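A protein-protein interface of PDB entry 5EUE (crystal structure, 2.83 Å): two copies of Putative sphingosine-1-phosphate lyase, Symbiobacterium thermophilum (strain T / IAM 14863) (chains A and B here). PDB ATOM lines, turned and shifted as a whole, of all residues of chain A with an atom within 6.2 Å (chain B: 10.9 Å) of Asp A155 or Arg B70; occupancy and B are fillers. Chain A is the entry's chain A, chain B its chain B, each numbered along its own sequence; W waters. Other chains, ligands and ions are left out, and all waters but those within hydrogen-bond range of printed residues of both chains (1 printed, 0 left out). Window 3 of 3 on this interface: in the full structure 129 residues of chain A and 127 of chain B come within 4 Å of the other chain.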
ATOM      1  N   GLU A 143      27.654  28.000 -23.170  1.00  0.00           N
ATOM      2  CA  GLU A 143      27.490  26.554 -23.229  1.00  0.00           C
ATOM      3  C   GLU A 143      26.744  26.099 -24.483  1.00  0.00           C
ATOM      4  O   GLU A 143      27.116  25.065 -25.051  1.00  0.00           O
ATOM      5  CB  GLU A 143      26.890  26.001 -21.947  1.00  0.00           C
ATOM      6  CG  GLU A 143      27.966  25.869 -20.885  1.00  0.00           C
ATOM      7  CD  GLU A 143      27.547  25.336 -19.535  1.00  0.00           C
ATOM      8  OE1 GLU A 143      26.442  24.762 -19.421  1.00  0.00           O
ATOM      9  OE2 GLU A 143      28.365  25.441 -18.595  1.00  0.00           O
ATOM     10  N   ALA A 146      29.437  26.501 -27.201  1.00  0.00           N
ATOM     11  CA  ALA A 146      30.413  25.431 -27.077  1.00  0.00           C
ATOM     12  C   ALA A 146      29.904  24.105 -27.676  1.00  0.00           C
ATOM     13  O   ALA A 146      30.629  23.470 -28.449  1.00  0.00           O
ATOM     14  CB  ALA A 146      30.775  25.241 -25.626  1.00  0.00           C
ATOM     15  N   MET A 147      28.648  23.720 -27.350  1.00  0.00           N
ATOM     16  CA  MET A 147      28.019  22.481 -27.800  1.00  0.00           C
ATOM     17  C   MET A 147      27.717  22.466 -29.307  1.00  0.00           C
ATOM     18  O   MET A 147      28.035  21.480 -29.981  1.00  0.00           O
ATOM     19  CB  MET A 147      26.770  22.170 -26.956  1.00  0.00           C
ATOM     20  CG  MET A 147      27.089  21.919 -25.507  1.00  0.00           C
ATOM     21  SD  MET A 147      25.692  21.420 -24.465  1.00  0.00           S
ATOM     22  CE  MET A 147      24.731  22.939 -24.396  1.00  0.00           C
ATOM     23  N   ALA A 149      29.112  24.332 -31.664  1.00  0.00           N
ATOM     24  CA  ALA A 149      30.435  24.364 -32.263  1.00  0.00           C
ATOM     25  C   ALA A 149      30.985  22.949 -32.415  1.00  0.00           C
ATOM     26  O   ALA A 149      31.389  22.581 -33.520  1.00  0.00           O
ATOM     27  CB  ALA A 149      31.358  25.203 -31.412  1.00  0.00           C
ATOM     28  N   HIS A 150      30.914  22.139 -31.330  1.00  0.00           N
ATOM     29  CA  HIS A 150      31.370  20.752 -31.267  1.00  0.00           C
ATOM     30  C   HIS A 150      30.663  19.862 -32.289  1.00  0.00           C
ATOM     31  O   HIS A 150      31.321  19.102 -33.007  1.00  0.00           O
ATOM     32  CB  HIS A 150      31.194  20.184 -29.849  1.00  0.00           C
ATOM     33  CG  HIS A 150      31.808  18.826 -29.687  1.00  0.00           C
ATOM     34  ND1 HIS A 150      31.037  17.687 -29.695  1.00  0.00           N
ATOM     35  CD2 HIS A 150      33.111  18.473 -29.570  1.00  0.00           C
ATOM     36  CE1 HIS A 150      31.883  16.680 -29.536  1.00  0.00           C
ATOM     37  NE2 HIS A 150      33.138  17.108 -29.444  1.00  0.00           N
ATOM     38  N   LEU A 152      29.347  20.916 -34.951  1.00  0.00           N
ATOM     39  CA  LEU A 152      29.677  21.370 -36.304  1.00  0.00           C
ATOM     40  C   LEU A 152      31.189  21.446 -36.534  1.00  0.00           C
ATOM     41  O   LEU A 152      31.713  22.438 -37.063  1.00  0.00           O
ATOM     42  CB  LEU A 152      28.950  22.680 -36.682  1.00  0.00           C
ATOM     43  CG  LEU A 152      27.433  22.675 -36.577  1.00  0.00           C
ATOM     44  CD1 LEU A 152      26.906  24.065 -36.553  1.00  0.00           C
ATOM     45  CD2 LEU A 152      26.806  21.916 -37.690  1.00  0.00           C
ATOM     46  N   GLY A 153      31.856  20.358 -36.145  1.00  0.00           N
ATOM     47  CA  GLY A 153      33.293  20.131 -36.313  1.00  0.00           C
ATOM     48  C   GLY A 153      34.261  21.147 -35.739  1.00  0.00           C
ATOM     49  O   GLY A 153      35.314  21.399 -36.337  1.00  0.00           O
ATOM     50  N   GLY A 154      33.923  21.699 -34.578  1.00  0.00           N
ATOM     51  CA  GLY A 154      34.748  22.687 -33.882  1.00  0.00           C
ATOM     52  C   GLY A 154      36.129  22.187 -33.510  1.00  0.00           C
ATOM     53  O   GLY A 154      37.111  22.909 -33.689  1.00  0.00           O
ATOM     54  N   ASP A 155      36.223  20.927 -33.028  1.00  0.00           N
ATOM     55  CA  ASP A 155      37.507  20.334 -32.636  1.00  0.00           C
ATOM     56  C   ASP A 155      38.518  20.299 -33.778  1.00  0.00           C
ATOM     57  O   ASP A 155      39.694  20.633 -33.568  1.00  0.00           O
ATOM     58  CB  ASP A 155      37.324  18.948 -32.036  1.00  0.00           C
ATOM     59  CG  ASP A 155      36.742  18.909 -30.640  1.00  0.00           C
ATOM     60  OD1 ASP A 155      36.277  17.823 -30.227  1.00  0.00           O
ATOM     61  OD2 ASP A 155      36.765  19.967 -29.946  1.00  0.00           O
ATOM     62  N   ALA A 156      38.033  19.958 -34.999  1.00  0.00           N
ATOM     63  CA  ALA A 156      38.792  19.885 -36.244  1.00  0.00           C
ATOM     64  C   ALA A 156      39.531  21.187 -36.531  1.00  0.00           C
ATOM     65  O   ALA A 156      40.703  21.146 -36.911  1.00  0.00           O
ATOM     66  CB  ALA A 156      37.861  19.543 -37.394  1.00  0.00           C
ATOM     67  N   ALA A 157      38.869  22.344 -36.287  1.00  0.00           N
ATOM     68  CA  ALA A 157      39.419  23.684 -36.521  1.00  0.00           C
ATOM     69  C   ALA A 157      40.442  24.166 -35.450  1.00  0.00           C
ATOM     70  O   ALA A 157      40.776  25.360 -35.392  1.00  0.00           O
ATOM     71  CB  ALA A 157      38.290  24.675 -36.688  1.00  0.00           C
ATOM     72  N   GLY A 158      40.978  23.231 -34.666  1.00  0.00           N
ATOM     73  CA  GLY A 158      42.009  23.508 -33.669  1.00  0.00           C
ATOM     74  C   GLY A 158      41.585  24.151 -32.365  1.00  0.00           C
ATOM     75  O   GLY A 158      42.405  24.795 -31.713  1.00  0.00           O
ATOM     76  N   GLY A 159      40.327  23.962 -31.973  1.00  0.00           N
ATOM     77  CA  GLY A 159      39.774  24.513 -30.739  1.00  0.00           C
ATOM     78  C   GLY A 159      39.700  26.030 -30.680  1.00  0.00           C
ATOM     79  O   GLY A 159      39.690  26.610 -29.592  1.00  0.00           O
ATOM     80  N   VAL A 161      37.287  27.709 -32.587  1.00  0.00           N
ATOM     81  CA  VAL A 161      35.912  28.040 -32.948  1.00  0.00           C
ATOM     82  C   VAL A 161      35.215  28.701 -31.754  1.00  0.00           C
ATOM     83  O   VAL A 161      35.126  28.136 -30.658  1.00  0.00           O
ATOM     84  CB  VAL A 161      35.111  26.854 -33.582  1.00  0.00           C
ATOM     85  CG1 VAL A 161      33.619  27.163 -33.708  1.00  0.00           C
ATOM     86  CG2 VAL A 161      35.676  26.494 -34.949  1.00  0.00           C
ATOM     87  N   LEU A 368      20.413  20.025 -23.852  1.00  0.00           N
ATOM     88  CA  LEU A 368      20.698  19.111 -22.753  1.00  0.00           C
ATOM     89  C   LEU A 368      19.645  18.048 -22.552  1.00  0.00           C
ATOM     90  O   LEU A 368      19.999  16.969 -22.094  1.00  0.00           O
ATOM     91  CB  LEU A 368      20.930  19.858 -21.445  1.00  0.00           C
ATOM     92  CG  LEU A 368      22.182  20.733 -21.385  1.00  0.00           C
ATOM     93  CD1 LEU A 368      22.224  21.435 -20.104  1.00  0.00           C
ATOM     94  CD2 LEU A 368      23.452  19.917 -21.538  1.00  0.00           C
ATOM     95  N   GLU A 372      22.905  13.893 -27.843  1.00  0.00           N
ATOM     96  CA  GLU A 372      23.215  13.289 -29.145  1.00  0.00           C
ATOM     97  C   GLU A 372      22.212  12.191 -29.571  1.00  0.00           C
ATOM     98  O   GLU A 372      21.924  12.053 -30.766  1.00  0.00           O
ATOM     99  CB  GLU A 372      24.659  12.774 -29.182  1.00  0.00           C
ATOM    100  CG  GLU A 372      25.711  13.833 -28.894  1.00  0.00           C
ATOM    101  CD  GLU A 372      27.140  13.472 -29.256  1.00  0.00           C
ATOM    102  OE1 GLU A 372      27.329  12.719 -30.237  1.00  0.00           O
ATOM    103  OE2 GLU A 372      28.071  14.005 -28.606  1.00  0.00           O
ATOM    104  N   PRO B  66      28.156  21.773 -13.172  1.00  0.00           N
ATOM    105  CA  PRO B  66      28.945  21.099 -14.216  1.00  0.00           C
ATOM    106  C   PRO B  66      28.826  21.815 -15.562  1.00  0.00           C
ATOM    107  O   PRO B  66      27.724  22.157 -15.999  1.00  0.00           O
ATOM    108  CB  PRO B  66      28.395  19.661 -14.241  1.00  0.00           C
ATOM    109  CG  PRO B  66      27.212  19.645 -13.303  1.00  0.00           C
ATOM    110  CD  PRO B  66      26.901  21.045 -12.886  1.00  0.00           C
ATOM    111  N   SER B  67      29.984  22.097 -16.173  1.00  0.00           N
ATOM    112  CA  SER B  67      30.116  22.753 -17.469  1.00  0.00           C
ATOM    113  C   SER B  67      29.605  21.824 -18.558  1.00  0.00           C
ATOM    114  O   SER B  67      29.708  20.598 -18.425  1.00  0.00           O
ATOM    115  CB  SER B  67      31.581  23.072 -17.748  1.00  0.00           C
ATOM    116  OG  SER B  67      32.362  21.886 -17.801  1.00  0.00           O
ATOM    117  N   HIS B  68      29.080  22.405 -19.643  1.00  0.00           N
ATOM    118  CA  HIS B  68      28.589  21.661 -20.797  1.00  0.00           C
ATOM    119  C   HIS B  68      29.221  22.222 -22.076  1.00  0.00           C
ATOM    120  O   HIS B  68      28.666  23.143 -22.696  1.00  0.00           O
ATOM    121  CB  HIS B  68      27.064  21.717 -20.852  1.00  0.00           C
ATOM    122  CG  HIS B  68      26.406  21.056 -19.685  1.00  0.00           C
ATOM    123  ND1 HIS B  68      26.436  19.679 -19.523  1.00  0.00           N
ATOM    124  CD2 HIS B  68      25.668  21.601 -18.689  1.00  0.00           C
ATOM    125  CE1 HIS B  68      25.716  19.434 -18.441  1.00  0.00           C
ATOM    126  NE2 HIS B  68      25.232  20.559 -17.906  1.00  0.00           N
ATOM    127  N   ALA B  69      30.412  21.716 -22.429  1.00  0.00           N
ATOM    128  CA  ALA B  69      31.127  22.164 -23.628  1.00  0.00           C
ATOM    129  C   ALA B  69      30.814  21.292 -24.846  1.00  0.00           C
ATOM    130  O   ALA B  69      31.221  21.613 -25.965  1.00  0.00           O
ATOM    131  CB  ALA B  69      32.626  22.182 -23.376  1.00  0.00           C
ATOM    132  N   ARG B  70      30.110  20.190 -24.619  1.00  0.00           N
ATOM    133  CA  ARG B  70      29.745  19.210 -25.628  1.00  0.00           C
ATOM    134  C   ARG B  70      28.367  18.708 -25.267  1.00  0.00           C
ATOM    135  O   ARG B  70      28.026  18.684 -24.083  1.00  0.00           O
ATOM    136  CB  ARG B  70      30.728  18.009 -25.586  1.00  0.00           C
ATOM    137  CG  ARG B  70      32.085  18.274 -26.241  1.00  0.00           C
ATOM    138  CD  ARG B  70      33.205  17.367 -25.744  1.00  0.00           C
ATOM    139  NE  ARG B  70      32.954  15.954 -26.041  1.00  0.00           N
ATOM    140  CZ  ARG B  70      33.698  15.218 -26.861  1.00  0.00           C
ATOM    141  NH1 ARG B  70      34.752  15.747 -27.467  1.00  0.00           N
ATOM    142  NH2 ARG B  70      33.392  13.946 -27.082  1.00  0.00           N
ATOM    143  N   LEU B  71      27.581  18.282 -26.258  1.00  0.00           N
ATOM    144  CA  LEU B  71      26.256  17.721 -26.000  1.00  0.00           C
ATOM    145  C   LEU B  71      26.434  16.423 -25.240  1.00  0.00           C
ATOM    146  O   LEU B  71      27.313  15.638 -25.627  1.00  0.00           O
ATOM    147  CB  LEU B  71      25.527  17.382 -27.317  1.00  0.00           C
ATOM    148  CG  LEU B  71      24.805  18.508 -28.003  1.00  0.00           C
ATOM    149  CD1 LEU B  71      24.510  18.149 -29.474  1.00  0.00           C
ATOM    150  CD2 LEU B  71      23.551  18.879 -27.245  1.00  0.00           C
ATOM    151  N   PRO B  72      25.619  16.130 -24.196  1.00  0.00           N
ATOM    152  CA  PRO B  72      25.746  14.825 -23.538  1.00  0.00           C
ATOM    153  C   PRO B  72      25.330  13.730 -24.524  1.00  0.00           C
ATOM    154  O   PRO B  72      24.608  14.049 -25.456  1.00  0.00           O
ATOM    155  CB  PRO B  72      24.798  14.944 -22.342  1.00  0.00           C
ATOM    156  CG  PRO B  72      23.821  15.953 -22.722  1.00  0.00           C
ATOM    157  CD  PRO B  72      24.528  16.929 -23.602  1.00  0.00           C
ATOM    158  N   ARG B  73      25.832  12.499 -24.391  1.00  0.00           N
ATOM    159  CA  ARG B  73      25.466  11.395 -25.300  1.00  0.00           C
ATOM    160  C   ARG B  73      23.941  11.178 -25.263  1.00  0.00           C
ATOM    161  O   ARG B  73      23.270  11.287 -26.292  1.00  0.00           O
ATOM    162  CB  ARG B  73      26.205  10.082 -24.945  1.00  0.00           C
ATOM    163  CG  ARG B  73      27.698  10.060 -25.281  1.00  0.00           C
ATOM    164  CD  ARG B  73      28.305   8.668 -25.113  1.00  0.00           C
ATOM    165  NE  ARG B  73      27.899   7.746 -26.181  1.00  0.00           N
ATOM    166  CZ  ARG B  73      26.933   6.838 -26.074  1.00  0.00           C
ATOM    167  NH1 ARG B  73      26.262   6.702 -24.933  1.00  0.00           N
ATOM    168  NH2 ARG B  73      26.629   6.061 -27.104  1.00  0.00           N
ATOM    169  N   ALA B  74      23.416  10.901 -24.060  1.00  0.00           N
ATOM    170  CA  ALA B  74      21.990  10.744 -23.802  1.00  0.00           C
ATOM    171  C   ALA B  74      21.519  12.044 -23.149  1.00  0.00           C
ATOM    172  O   ALA B  74      22.299  12.717 -22.461  1.00  0.00           O
ATOM    173  CB  ALA B  74      21.749   9.568 -22.868  1.00  0.00           C
ATOM    174  N   GLY B  75      20.276  12.419 -23.415  1.00  0.00           N
ATOM    175  CA  GLY B  75      19.710  13.634 -22.860  1.00  0.00           C
ATOM    176  C   GLY B  75      19.537  13.526 -21.369  1.00  0.00           C
ATOM    177  O   GLY B  75      19.215  12.456 -20.865  1.00  0.00           O
ATOM    178  N   LEU B  76      19.809  14.606 -20.653  1.00  0.00           N
ATOM    179  CA  LEU B  76      19.644  14.668 -19.202  1.00  0.00           C
ATOM    180  C   LEU B  76      18.146  14.757 -18.853  1.00  0.00           C
ATOM    181  O   LEU B  76      17.389  15.367 -19.627  1.00  0.00           O
ATOM    182  CB  LEU B  76      20.367  15.908 -18.634  1.00  0.00           C
ATOM    183  CG  LEU B  76      21.888  15.939 -18.758  1.00  0.00           C
ATOM    184  CD1 LEU B  76      22.373  17.335 -18.783  1.00  0.00           C
ATOM    185  CD2 LEU B  76      22.555  15.178 -17.637  1.00  0.00           C
ATOM    186  N   VAL B 508      34.381  28.676 -21.840  1.00  0.00           N
ATOM    187  CA  VAL B 508      33.976  27.428 -21.168  1.00  0.00           C
ATOM    188  C   VAL B 508      35.259  26.777 -20.585  1.00  0.00           C
ATOM    189  O   VAL B 508      36.085  26.236 -21.331  1.00  0.00           O
ATOM    190  CB  VAL B 508      33.068  26.454 -21.992  1.00  0.00           C
ATOM    191  CG1 VAL B 508      32.605  25.281 -21.134  1.00  0.00           C
ATOM    192  CG2 VAL B 508      31.850  27.172 -22.552  1.00  0.00           C
ATOM    193  N   HIS B 509      35.444  26.923 -19.257  1.00  0.00           N
ATOM    194  CA  HIS B 509      36.580  26.404 -18.491  1.00  0.00           C
ATOM    195  C   HIS B 509      36.121  25.915 -17.114  1.00  0.00           C
ATOM    196  O   HIS B 509      34.925  25.736 -16.878  1.00  0.00           O
ATOM    197  CB  HIS B 509      37.666  27.482 -18.335  1.00  0.00           C
ATOM    198  CG  HIS B 509      38.551  27.635 -19.533  1.00  0.00           C
ATOM    199  ND1 HIS B 509      38.125  28.309 -20.668  1.00  0.00           N
ATOM    200  CD2 HIS B 509      39.824  27.214 -19.728  1.00  0.00           C
ATOM    201  CE1 HIS B 509      39.141  28.263 -21.516  1.00  0.00           C
ATOM    202  NE2 HIS B 509      40.187  27.617 -20.994  1.00  0.00           N
HETATM  203  O   HOH W   1      28.159  18.822 -28.975  1.00  0.00           O
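OE2 of Glu A143 touches CA of Ser B67 (3.4 Å). Val B508 touches Ala A146. Met A147 touches His B68 (CG to O, 3.4 Å). Met A147 touches Ala B69 (N to O, 3.6 Å). Met A147 touches Leu B71 (CG to N, 3.7 Å). Leu A368 touches His B68. Pro B72 touches Leu A368. O of Leu A368 touches CA of Gly B75 (3.4 Å).
Of the printed residues of chain B, Ala A146 touches Ala B69 and Val B508. Of the printed residues of chain B, Met A147 touches His B68, Ala B69, Arg B70 and Leu B71. Ala A149 touches none of the printed residues of chain B. His A150 touches just one residue of chain B: Arg B70 (2.9 Å). Gly A154 touches none of the printed residues of chain B. No residue of chain B comes within 4 Å of Ala A156. No residue of chain B comes within 4 Å of Ala A157. Arg B70 touches just these residues of chain A: Met A147 (3.5 Å), His A150 (2.9 Å) and Asp A155 (3.8 Å). Of the printed residues of chain A, Pro B72 touches Leu A368 and Glu A372. Of the printed residues of chain A, Gly B75 touches Leu A368. Of the printed residues of chain A, Leu B76 touches Leu A368 (2.8 Å). The nearest residue of chain B that does not touch Asp A155 is Ala B69 (7.0 Å). The nearest printed residue of chain B that does not touch Ala A146 is His B68 (4.2 Å).
Of the 16 printed residues of chain A, 7 touch a printed residue of chain B. Hydrophobic or aromatic side chains of chain A that line the printed part of chain B: Ala A146, Met A147, His A150 and Leu A368. Printed residues of chain B that touch a printed residue of chain A: Ser B67, His B68, Ala B69, Arg B70, Leu B71, Pro B72, Arg B73, Gly B75, Leu B76 and Val B508. Hydrophobic or aromatic side chains of chain B within 4 Å of the printed part of chain A: His B68, Leu B71, Pro B72, Leu B76 and Val B508. Among the printed residues, 17 pairs touch across the chains.
A ring nitrogen (NE2) of His A150 sits close to the side-chain carboxylate of Asp A155 (3.3 Å).
The backbone NH (N) of His B68 is in hydrogen-bond range of the side-chain carboxylate (OE2) of Glu A143. A ring nitrogen (NE2) of His A150 is in hydrogen-bond range of the guanidinium group (NH1) of Arg B70 (2.9 Å). The guanidinium group (NH1) of Arg B70 lies within salt-bridge range of the side-chain carboxylate (OD1) of Asp A155 (3.8 Å). The backbone carbonyl oxygen (O) of Leu A368 lies within hydrogen-bond range of the backbone NH (N) of Leu B76, at 2.8 Å. The backbone NH (N) of Glu A372 lies within hydrogen-bond range of the backbone carbonyl oxygen (O) of Pro B72 (2.9 Å). O of Arg B73 lies within hydrogen-bond range of N of Glu A372 (3.1 Å). The backbone carbonyl oxygen of Ala B69 sits close to the backbone carbonyl oxygen of Ala A146, at 3.2 Å. The backbone carbonyl oxygen (O) of Arg B70 lies close to the side-chain sulfur (SD) of Met A147, 3.6 Å away. O of Leu B71 lies close to OE2 of Glu A372 (3.5 Å).
Water W1 lies within hydrogen-bond range of the backbone NH of Leu B71 (2.8 Å), the backbone carbonyl oxygen of Met A147 (2.8 Å) and a ring nitrogen (ND1) of His A150 (3.2 Å).
No position is printed for both chains.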
